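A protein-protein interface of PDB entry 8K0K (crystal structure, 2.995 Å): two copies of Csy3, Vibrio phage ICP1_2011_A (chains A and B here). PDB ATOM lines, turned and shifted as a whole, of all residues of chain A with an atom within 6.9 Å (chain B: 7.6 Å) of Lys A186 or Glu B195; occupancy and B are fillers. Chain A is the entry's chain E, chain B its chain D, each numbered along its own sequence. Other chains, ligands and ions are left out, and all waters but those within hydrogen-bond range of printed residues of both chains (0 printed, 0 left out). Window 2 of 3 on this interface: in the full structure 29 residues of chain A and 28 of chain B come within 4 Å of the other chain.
Of the 17 printed residues of chain B, 4 touch a printed residue of chain A. Along chain A the printed residues that touch a printed residue of chain B span positions 19 to 186. Among the printed residues, Asp or Glu carboxylates within 4 Å of a Lys or Arg side-chain nitrogen of the other chain: Lys A186 with Glu B195 (3.3 Å).
The side-chain amino group of Lys A186 is in salt-bridge range of the side-chain carboxylate of Glu B195, at 3.3 Å. NE2 of His B72 is in hydrogen-bond range of O of Asn A20, 2.9 Å away.
No position is printed for both chains. Of the 7 pairs that touch across the chains among the printed residues, none has its exchanged pair printed and touching as well.
The side-chain amide nitrogen (ND2) of Asn B69 lies close to the backbone NH (N) of Glu B198 (3.4 Å). ND2 of Asn B69 sits at hydrogen-bond distance from O of Gly B196, 2.8 Å away. O of Pro B71 lies within hydrogen-bond range of N of Gly B196, 2.8 Å away. The backbone NH (N) of Thr A144 is in hydrogen-bond range of the backbone carbonyl oxygen (O) of Lys A186 (2.9 Å). The backbone NH of Thr A19 is in hydrogen-bond range of the backbone carbonyl oxygen of Asn A82. N of Gly B196 sits close to O of Leu B70, at 3.4 Å.
His B72 touches Thr A19 (NE2 to OG1, 3.8 Å). Thr A19 touches Glu B195. Thr A19 touches Gly B196. Asn A20 touches Asn B69. Asn A82 touches Glu B195.
Printed residues of chain B within 4 Å of Thr A19: His B72, Glu B195 and Gly B196. Thr A184 touches none of the printed residues of chain B. Lys A186 touches one residue of chain B. Asn B27 touches none of the printed residues of chain A. Printed residues of chain A within 4 Å of Asn B69: Asn A20 (3.6 Å). Glu B195 touches three residues of chain A. The nearest residue of chain B that does not touch Lys A186 is Gly B194 (5.6 Å). The nearest residue of chain A that does not touch Glu B195 is Tyr A81 (6.5 Å). The nearest printed residue of chain B that does not touch Thr A19 is Ser B197 (4.3 Å).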
ATOM      1  N   THR A  19      12.230 -30.716 -14.764  1.00  0.00           N
ATOM      2  CA  THR A  19      13.470 -30.795 -14.014  1.00  0.00           C
ATOM      3  C   THR A  19      13.166 -30.872 -12.523  1.00  0.00           C
ATOM      4  O   THR A  19      12.016 -30.771 -12.093  1.00  0.00           O
ATOM      5  CB  THR A  19      14.352 -29.581 -14.299  1.00  0.00           C
ATOM      6  OG1 THR A  19      13.712 -28.409 -13.784  1.00  0.00           O
ATOM      7  CG2 THR A  19      14.569 -29.414 -15.792  1.00  0.00           C
ATOM      8  N   ASN A  20      14.216 -31.067 -11.727  1.00  0.00           N
ATOM      9  CA  ASN A  20      14.087 -30.827 -10.299  1.00  0.00           C
ATOM     10  C   ASN A  20      13.771 -29.353 -10.061  1.00  0.00           C
ATOM     11  O   ASN A  20      14.157 -28.481 -10.846  1.00  0.00           O
ATOM     12  CB  ASN A  20      15.372 -31.216  -9.566  1.00  0.00           C
ATOM     13  CG  ASN A  20      15.738 -32.674  -9.756  1.00  0.00           C
ATOM     14  OD1 ASN A  20      14.877 -33.527  -9.970  1.00  0.00           O
ATOM     15  ND2 ASN A  20      17.028 -32.969  -9.672  1.00  0.00           N
ATOM     16  N   TYR A  81      11.797 -24.266 -11.851  1.00  0.00           N
ATOM     17  CA  TYR A  81      12.065 -25.482 -12.620  1.00  0.00           C
ATOM     18  C   TYR A  81      11.772 -25.227 -14.094  1.00  0.00           C
ATOM     19  O   TYR A  81      11.377 -24.130 -14.492  1.00  0.00           O
ATOM     20  CB  TYR A  81      11.260 -26.679 -12.099  1.00  0.00           C
ATOM     21  CG  TYR A  81       9.767 -26.469 -12.055  1.00  0.00           C
ATOM     22  CD1 TYR A  81       9.160 -25.959 -10.919  1.00  0.00           C
ATOM     23  CD2 TYR A  81       8.963 -26.800 -13.139  1.00  0.00           C
ATOM     24  CE1 TYR A  81       7.799 -25.769 -10.863  1.00  0.00           C
ATOM     25  CE2 TYR A  81       7.593 -26.612 -13.090  1.00  0.00           C
ATOM     26  CZ  TYR A  81       7.021 -26.096 -11.945  1.00  0.00           C
ATOM     27  OH  TYR A  81       5.665 -25.898 -11.869  1.00  0.00           O
ATOM     28  N   ASN A  82      12.006 -26.252 -14.911  1.00  0.00           N
ATOM     29  CA  ASN A  82      11.700 -26.226 -16.333  1.00  0.00           C
ATOM     30  C   ASN A  82      10.907 -27.473 -16.697  1.00  0.00           C
ATOM     31  O   ASN A  82      11.054 -28.525 -16.071  1.00  0.00           O
ATOM     32  CB  ASN A  82      12.965 -26.166 -17.197  1.00  0.00           C
ATOM     33  CG  ASN A  82      13.676 -24.838 -17.109  1.00  0.00           C
ATOM     34  OD1 ASN A  82      13.110 -23.845 -16.660  1.00  0.00           O
ATOM     35  ND2 ASN A  82      14.928 -24.811 -17.549  1.00  0.00           N
ATOM     36  N   VAL A  83      10.071 -27.350 -17.722  1.00  0.00           N
ATOM     37  CA  VAL A  83       9.246 -28.449 -18.207  1.00  0.00           C
ATOM     38  C   VAL A  83       9.403 -28.496 -19.718  1.00  0.00           C
ATOM     39  O   VAL A  83       8.935 -27.592 -20.416  1.00  0.00           O
ATOM     40  CB  VAL A  83       7.771 -28.278 -17.823  1.00  0.00           C
ATOM     41  CG1 VAL A  83       6.967 -29.472 -18.287  1.00  0.00           C
ATOM     42  CG2 VAL A  83       7.626 -28.079 -16.326  1.00  0.00           C
ATOM     43  N   VAL A 142       5.236 -17.364 -13.138  1.00  0.00           N
ATOM     44  CA  VAL A 142       5.842 -16.767 -14.322  1.00  0.00           C
ATOM     45  C   VAL A 142       6.355 -17.889 -15.214  1.00  0.00           C
ATOM     46  O   VAL A 142       7.226 -18.668 -14.803  1.00  0.00           O
ATOM     47  CB  VAL A 142       6.976 -15.800 -13.956  1.00  0.00           C
ATOM     48  CG1 VAL A 142       7.571 -15.195 -15.207  1.00  0.00           C
ATOM     49  CG2 VAL A 142       6.459 -14.715 -13.027  1.00  0.00           C
ATOM     50  N   ILE A 143       5.826 -17.958 -16.432  1.00  0.00           N
ATOM     51  CA  ILE A 143       6.196 -18.973 -17.417  1.00  0.00           C
ATOM     52  C   ILE A 143       6.811 -18.266 -18.619  1.00  0.00           C
ATOM     53  O   ILE A 143       6.171 -17.401 -19.229  1.00  0.00           O
ATOM     54  CB  ILE A 143       4.985 -19.817 -17.846  1.00  0.00           C
ATOM     55  CG1 ILE A 143       4.244 -20.360 -16.625  1.00  0.00           C
ATOM     56  CG2 ILE A 143       5.418 -20.959 -18.755  1.00  0.00           C
ATOM     57  CD1 ILE A 143       3.059 -21.242 -16.975  1.00  0.00           C
ATOM     58  N   THR A 144       8.054 -18.605 -18.948  1.00  0.00           N
ATOM     59  CA  THR A 144       8.716 -18.020 -20.138  1.00  0.00           C
ATOM     60  C   THR A 144       8.860 -19.104 -21.207  1.00  0.00           C
ATOM     61  O   THR A 144       9.436 -20.147 -20.904  1.00  0.00           O
ATOM     62  CB  THR A 144      10.054 -17.367 -19.777  1.00  0.00           C
ATOM     63  OG1 THR A 144       9.798 -16.293 -18.875  1.00  0.00           O
ATOM     64  CG2 THR A 144      10.797 -16.849 -20.987  1.00  0.00           C
ATOM     65  N   VAL A 145       8.326 -18.853 -22.399  1.00  0.00           N
ATOM     66  CA  VAL A 145       8.382 -19.824 -23.526  1.00  0.00           C
ATOM     67  C   VAL A 145       8.708 -19.049 -24.804  1.00  0.00           C
ATOM     68  O   VAL A 145       7.979 -18.109 -25.123  1.00  0.00           O
ATOM     69  CB  VAL A 145       7.057 -20.590 -23.656  1.00  0.00           C
ATOM     70  CG1 VAL A 145       5.855 -19.665 -23.586  1.00  0.00           C
ATOM     71  CG2 VAL A 145       7.020 -21.443 -24.911  1.00  0.00           C
ATOM     72  N   ASN A 146       9.774 -19.433 -25.498  1.00  0.00           N
ATOM     73  CA  ASN A 146      10.189 -18.744 -26.749  1.00  0.00           C
ATOM     74  C   ASN A 146      10.352 -17.252 -26.459  1.00  0.00           C
ATOM     75  O   ASN A 146       9.699 -16.444 -27.132  1.00  0.00           O
ATOM     76  CB  ASN A 146       9.234 -19.004 -27.919  1.00  0.00           C
ATOM     77  CG  ASN A 146       9.273 -20.426 -28.429  1.00  0.00           C
ATOM     78  OD1 ASN A 146      10.339 -20.949 -28.743  1.00  0.00           O
ATOM     79  ND2 ASN A 146       8.116 -21.060 -28.509  1.00  0.00           N
ATOM     80  N   THR A 184      10.282 -25.965 -24.326  1.00  0.00           N
ATOM     81  CA  THR A 184      10.594 -25.859 -22.906  1.00  0.00           C
ATOM     82  C   THR A 184       9.905 -24.636 -22.315  1.00  0.00           C
ATOM     83  O   THR A 184      10.129 -23.512 -22.775  1.00  0.00           O
ATOM     84  CB  THR A 184      12.103 -25.762 -22.680  1.00  0.00           C
ATOM     85  OG1 THR A 184      12.752 -26.931 -23.198  1.00  0.00           O
ATOM     86  CG2 THR A 184      12.403 -25.626 -21.194  1.00  0.00           C
ATOM     87  N   LEU A 185       9.070 -24.855 -21.300  1.00  0.00           N
ATOM     88  CA  LEU A 185       8.579 -23.777 -20.454  1.00  0.00           C
ATOM     89  C   LEU A 185       9.533 -23.626 -19.277  1.00  0.00           C
ATOM     90  O   LEU A 185       9.901 -24.619 -18.646  1.00  0.00           O
ATOM     91  CB  LEU A 185       7.167 -24.058 -19.942  1.00  0.00           C
ATOM     92  CG  LEU A 185       6.141 -24.798 -20.804  1.00  0.00           C
ATOM     93  CD1 LEU A 185       4.784 -24.764 -20.119  1.00  0.00           C
ATOM     94  CD2 LEU A 185       6.045 -24.223 -22.202  1.00  0.00           C
ATOM     95  N   LYS A 186       9.945 -22.393 -18.995  1.00  0.00           N
ATOM     96  CA  LYS A 186      10.827 -22.084 -17.876  1.00  0.00           C
ATOM     97  C   LYS A 186       9.994 -21.377 -16.813  1.00  0.00           C
ATOM     98  O   LYS A 186       9.466 -20.288 -17.062  1.00  0.00           O
ATOM     99  CB  LYS A 186      12.002 -21.226 -18.343  1.00  0.00           C
ATOM    100  CG  LYS A 186      12.496 -21.609 -19.741  1.00  0.00           C
ATOM    101  CD  LYS A 186      13.940 -21.186 -20.006  1.00  0.00           C
ATOM    102  CE  LYS A 186      14.907 -21.951 -19.105  1.00  0.00           C
ATOM    103  NZ  LYS A 186      16.301 -22.007 -19.639  1.00  0.00           N
ATOM    104  N   VAL A 187       9.858 -22.003 -15.640  1.00  0.00           N
ATOM    105  CA  VAL A 187       8.817 -21.675 -14.676  1.00  0.00           C
ATOM    106  C   VAL A 187       9.436 -21.181 -13.376  1.00  0.00           C
ATOM    107  O   VAL A 187      10.388 -21.782 -12.854  1.00  0.00           O
ATOM    108  CB  VAL A 187       7.923 -22.900 -14.405  1.00  0.00           C
ATOM    109  CG1 VAL A 187       6.808 -22.541 -13.439  1.00  0.00           C
ATOM    110  CG2 VAL A 187       7.376 -23.442 -15.707  1.00  0.00           C
ATOM    111  N   GLU A 188       8.866 -20.097 -12.847  1.00  0.00           N
ATOM    112  CA  GLU A 188       9.140 -19.615 -11.502  1.00  0.00           C
ATOM    113  C   GLU A 188       7.820 -19.414 -10.768  1.00  0.00           C
ATOM    114  O   GLU A 188       6.827 -18.983 -11.361  1.00  0.00           O
ATOM    115  CB  GLU A 188       9.916 -18.297 -11.512  1.00  0.00           C
ATOM    116  CG  GLU A 188      11.083 -18.249 -12.475  1.00  0.00           C
ATOM    117  CD  GLU A 188      11.806 -16.918 -12.424  1.00  0.00           C
ATOM    118  OE1 GLU A 188      13.044 -16.919 -12.239  1.00  0.00           O
ATOM    119  OE2 GLU A 188      11.132 -15.872 -12.556  1.00  0.00           O
ATOM    120  N   ASN B  27      28.248 -24.440 -20.374  1.00  0.00           N
ATOM    121  CA  ASN B  27      27.316 -23.574 -21.076  1.00  0.00           C
ATOM    122  C   ASN B  27      27.672 -23.553 -22.556  1.00  0.00           C
ATOM    123  O   ASN B  27      28.844 -23.634 -22.930  1.00  0.00           O
ATOM    124  CB  ASN B  27      27.329 -22.166 -20.493  1.00  0.00           C
ATOM    125  CG  ASN B  27      26.385 -22.023 -19.324  1.00  0.00           C
ATOM    126  OD1 ASN B  27      25.222 -22.426 -19.400  1.00  0.00           O
ATOM    127  ND2 ASN B  27      26.879 -21.462 -18.226  1.00  0.00           N
ATOM    128  N   ASN B  69      21.703 -35.144 -13.462  1.00  0.00           N
ATOM    129  CA  ASN B  69      21.164 -33.911 -14.016  1.00  0.00           C
ATOM    130  C   ASN B  69      22.290 -32.934 -14.324  1.00  0.00           C
ATOM    131  O   ASN B  69      23.304 -32.879 -13.622  1.00  0.00           O
ATOM    132  CB  ASN B  69      20.188 -33.232 -13.039  1.00  0.00           C
ATOM    133  CG  ASN B  69      18.820 -33.873 -13.033  1.00  0.00           C
ATOM    134  OD1 ASN B  69      18.571 -34.834 -12.302  1.00  0.00           O
ATOM    135  ND2 ASN B  69      17.908 -33.329 -13.841  1.00  0.00           N
ATOM    136  N   LEU B  70      22.098 -32.150 -15.380  1.00  0.00           N
ATOM    137  CA  LEU B  70      22.869 -30.930 -15.512  1.00  0.00           C
ATOM    138  C   LEU B  70      22.493 -29.994 -14.367  1.00  0.00           C
ATOM    139  O   LEU B  70      21.346 -29.994 -13.913  1.00  0.00           O
ATOM    140  CB  LEU B  70      22.592 -30.250 -16.850  1.00  0.00           C
ATOM    141  CG  LEU B  70      22.815 -31.066 -18.118  1.00  0.00           C
ATOM    142  CD1 LEU B  70      22.434 -30.235 -19.323  1.00  0.00           C
ATOM    143  CD2 LEU B  70      24.262 -31.545 -18.228  1.00  0.00           C
ATOM    144  N   PRO B  71      23.435 -29.200 -13.869  1.00  0.00           N
ATOM    145  CA  PRO B  71      23.087 -28.194 -12.859  1.00  0.00           C
ATOM    146  C   PRO B  71      22.059 -27.205 -13.391  1.00  0.00           C
ATOM    147  O   PRO B  71      21.699 -27.194 -14.568  1.00  0.00           O
ATOM    148  CB  PRO B  71      24.425 -27.515 -12.549  1.00  0.00           C
ATOM    149  CG  PRO B  71      25.364 -27.970 -13.610  1.00  0.00           C
ATOM    150  CD  PRO B  71      24.887 -29.300 -14.068  1.00  0.00           C
ATOM    151  N   HIS B  72      21.561 -26.367 -12.490  1.00  0.00           N
ATOM    152  CA  HIS B  72      20.606 -25.346 -12.887  1.00  0.00           C
ATOM    153  C   HIS B  72      21.281 -24.075 -13.383  1.00  0.00           C
ATOM    154  O   HIS B  72      20.591 -23.091 -13.669  1.00  0.00           O
ATOM    155  CB  HIS B  72      19.647 -25.038 -11.734  1.00  0.00           C
ATOM    156  CG  HIS B  72      18.530 -26.032 -11.605  1.00  0.00           C
ATOM    157  ND1 HIS B  72      18.709 -27.289 -11.065  1.00  0.00           N
ATOM    158  CD2 HIS B  72      17.227 -25.963 -11.971  1.00  0.00           C
ATOM    159  CE1 HIS B  72      17.563 -27.947 -11.093  1.00  0.00           C
ATOM    160  NE2 HIS B  72      16.647 -27.164 -11.638  1.00  0.00           N
ATOM    161  N   ASN B  73      22.609 -24.078 -13.511  1.00  0.00           N
ATOM    162  CA  ASN B  73      23.339 -22.948 -14.071  1.00  0.00           C
ATOM    163  C   ASN B  73      24.180 -23.339 -15.282  1.00  0.00           C
ATOM    164  O   ASN B  73      24.966 -22.516 -15.767  1.00  0.00           O
ATOM    165  CB  ASN B  73      24.220 -22.295 -13.001  1.00  0.00           C
ATOM    166  CG  ASN B  73      25.320 -23.208 -12.518  1.00  0.00           C
ATOM    167  OD1 ASN B  73      25.209 -24.429 -12.611  1.00  0.00           O
ATOM    168  ND2 ASN B  73      26.394 -22.622 -11.997  1.00  0.00           N
ATOM    169  N   LYS B  74      24.043 -24.570 -15.775  1.00  0.00           N
ATOM    170  CA  LYS B  74      24.666 -25.011 -17.015  1.00  0.00           C
ATOM    171  C   LYS B  74      23.590 -25.631 -17.895  1.00  0.00           C
ATOM    172  O   LYS B  74      22.713 -26.344 -17.401  1.00  0.00           O
ATOM    173  CB  LYS B  74      25.789 -26.027 -16.762  1.00  0.00           C
ATOM    174  CG  LYS B  74      26.863 -25.569 -15.780  1.00  0.00           C
ATOM    175  CD  LYS B  74      27.521 -24.276 -16.225  1.00  0.00           C
ATOM    176  CE  LYS B  74      28.575 -23.814 -15.232  1.00  0.00           C
ATOM    177  NZ  LYS B  74      29.786 -24.683 -15.250  1.00  0.00           N
ATOM    178  N   ASN B  75      23.649 -25.355 -19.200  1.00  0.00           N
ATOM    179  CA  ASN B  75      22.602 -25.788 -20.117  1.00  0.00           C
ATOM    180  C   ASN B  75      23.066 -26.790 -21.163  1.00  0.00           C
ATOM    181  O   ASN B  75      22.263 -27.176 -22.024  1.00  0.00           O
ATOM    182  CB  ASN B  75      21.979 -24.577 -20.827  1.00  0.00           C
ATOM    183  CG  ASN B  75      22.996 -23.767 -21.621  1.00  0.00           C
ATOM    184  OD1 ASN B  75      24.123 -24.204 -21.859  1.00  0.00           O
ATOM    185  ND2 ASN B  75      22.593 -22.575 -22.038  1.00  0.00           N
ATOM    186  N   THR B  76      24.323 -27.227 -21.125  1.00  0.00           N
ATOM    187  CA  THR B  76      24.859 -28.076 -22.178  1.00  0.00           C
ATOM    188  C   THR B  76      25.547 -29.291 -21.572  1.00  0.00           C
ATOM    189  O   THR B  76      26.361 -29.159 -20.654  1.00  0.00           O
ATOM    190  CB  THR B  76      25.828 -27.290 -23.071  1.00  0.00           C
ATOM    191  OG1 THR B  76      25.100 -26.273 -23.765  1.00  0.00           O
ATOM    192  CG2 THR B  76      26.494 -28.200 -24.091  1.00  0.00           C
ATOM    193  N   GLU B 137      18.382 -28.589 -28.586  1.00  0.00           N
ATOM    194  CA  GLU B 137      18.270 -27.441 -29.480  1.00  0.00           C
ATOM    195  C   GLU B 137      19.267 -27.543 -30.623  1.00  0.00           C
ATOM    196  O   GLU B 137      18.984 -27.099 -31.742  1.00  0.00           O
ATOM    197  CB  GLU B 137      18.493 -26.137 -28.716  1.00  0.00           C
ATOM    198  CG  GLU B 137      17.231 -25.403 -28.320  1.00  0.00           C
ATOM    199  CD  GLU B 137      17.509 -23.955 -27.957  1.00  0.00           C
ATOM    200  OE1 GLU B 137      18.416 -23.352 -28.572  1.00  0.00           O
ATOM    201  OE2 GLU B 137      16.828 -23.420 -27.055  1.00  0.00           O
ATOM    202  N   LEU B 192      22.782 -28.966 -26.393  1.00  0.00           N
ATOM    203  CA  LEU B 192      22.042 -27.890 -25.736  1.00  0.00           C
ATOM    204  C   LEU B 192      20.719 -28.475 -25.264  1.00  0.00           C
ATOM    205  O   LEU B 192      19.724 -28.479 -25.991  1.00  0.00           O
ATOM    206  CB  LEU B 192      21.838 -26.710 -26.676  1.00  0.00           C
ATOM    207  CG  LEU B 192      21.275 -25.445 -26.024  1.00  0.00           C
ATOM    208  CD1 LEU B 192      22.183 -24.974 -24.899  1.00  0.00           C
ATOM    209  CD2 LEU B 192      21.100 -24.348 -27.052  1.00  0.00           C
ATOM    210  N   LEU B 193      20.712 -28.984 -24.031  1.00  0.00           N
ATOM    211  CA  LEU B 193      19.531 -29.626 -23.465  1.00  0.00           C
ATOM    212  C   LEU B 193      18.678 -28.693 -22.624  1.00  0.00           C
ATOM    213  O   LEU B 193      17.455 -28.855 -22.591  1.00  0.00           O
ATOM    214  CB  LEU B 193      19.942 -30.829 -22.610  1.00  0.00           C
ATOM    215  CG  LEU B 193      20.604 -31.973 -23.378  1.00  0.00           C
ATOM    216  CD1 LEU B 193      21.216 -32.980 -22.431  1.00  0.00           C
ATOM    217  CD2 LEU B 193      19.595 -32.647 -24.281  1.00  0.00           C
ATOM    218  N   GLY B 194      19.280 -27.724 -21.961  1.00  0.00           N
ATOM    219  CA  GLY B 194      18.583 -26.893 -21.005  1.00  0.00           C
ATOM    220  C   GLY B 194      19.120 -27.104 -19.598  1.00  0.00           C
ATOM    221  O   GLY B 194      19.609 -28.185 -19.240  1.00  0.00           O
ATOM    222  N   GLU B 195      19.044 -26.053 -18.790  1.00  0.00           N
ATOM    223  CA  GLU B 195      19.517 -26.141 -17.417  1.00  0.00           C
ATOM    224  C   GLU B 195      18.669 -27.132 -16.633  1.00  0.00           C
ATOM    225  O   GLU B 195      17.439 -27.119 -16.716  1.00  0.00           O
ATOM    226  CB  GLU B 195      19.462 -24.774 -16.745  1.00  0.00           C
ATOM    227  CG  GLU B 195      19.798 -23.619 -17.653  1.00  0.00           C
ATOM    228  CD  GLU B 195      19.371 -22.297 -17.062  1.00  0.00           C
ATOM    229  OE1 GLU B 195      18.146 -22.062 -16.956  1.00  0.00           O
ATOM    230  OE2 GLU B 195      20.259 -21.499 -16.687  1.00  0.00           O
ATOM    231  N   GLY B 196      19.335 -27.994 -15.866  1.00  0.00           N
ATOM    232  CA  GLY B 196      18.644 -28.970 -15.047  1.00  0.00           C
ATOM    233  C   GLY B 196      18.144 -30.199 -15.772  1.00  0.00           C
ATOM    234  O   GLY B 196      17.339 -30.947 -15.205  1.00  0.00           O
ATOM    235  N   SER B 197      18.598 -30.445 -16.994  1.00  0.00           N
ATOM    236  CA  SER B 197      18.078 -31.557 -17.773  1.00  0.00           C
ATOM    237  C   SER B 197      18.593 -32.893 -17.253  1.00  0.00           C
ATOM    238  O   SER B 197      19.774 -33.042 -16.926  1.00  0.00           O
ATOM    239  CB  SER B 197      18.455 -31.400 -19.244  1.00  0.00           C
ATOM    240  OG  SER B 197      17.685 -30.383 -19.855  1.00  0.00           O
ATOM    241  N   GLU B 198      17.691 -33.865 -17.183  1.00  0.00           N
ATOM    242  CA  GLU B 198      18.082 -35.245 -16.945  1.00  0.00           C
ATOM    243  C   GLU B 198      19.005 -35.725 -18.060  1.00  0.00           C
ATOM    244  O   GLU B 198      18.722 -35.533 -19.247  1.00  0.00           O
ATOM    245  CB  GLU B 198      16.830 -36.118 -16.862  1.00  0.00           C
ATOM    246  CG  GLU B 198      17.063 -37.620 -16.830  1.00  0.00           C
ATOM    247  CD  GLU B 198      15.761 -38.397 -16.993  1.00  0.00           C
ATOM    248  OE1 GLU B 198      14.747 -37.778 -17.388  1.00  0.00           O
ATOM    249  OE2 GLU B 198      15.743 -39.619 -16.725  1.00  0.00           O
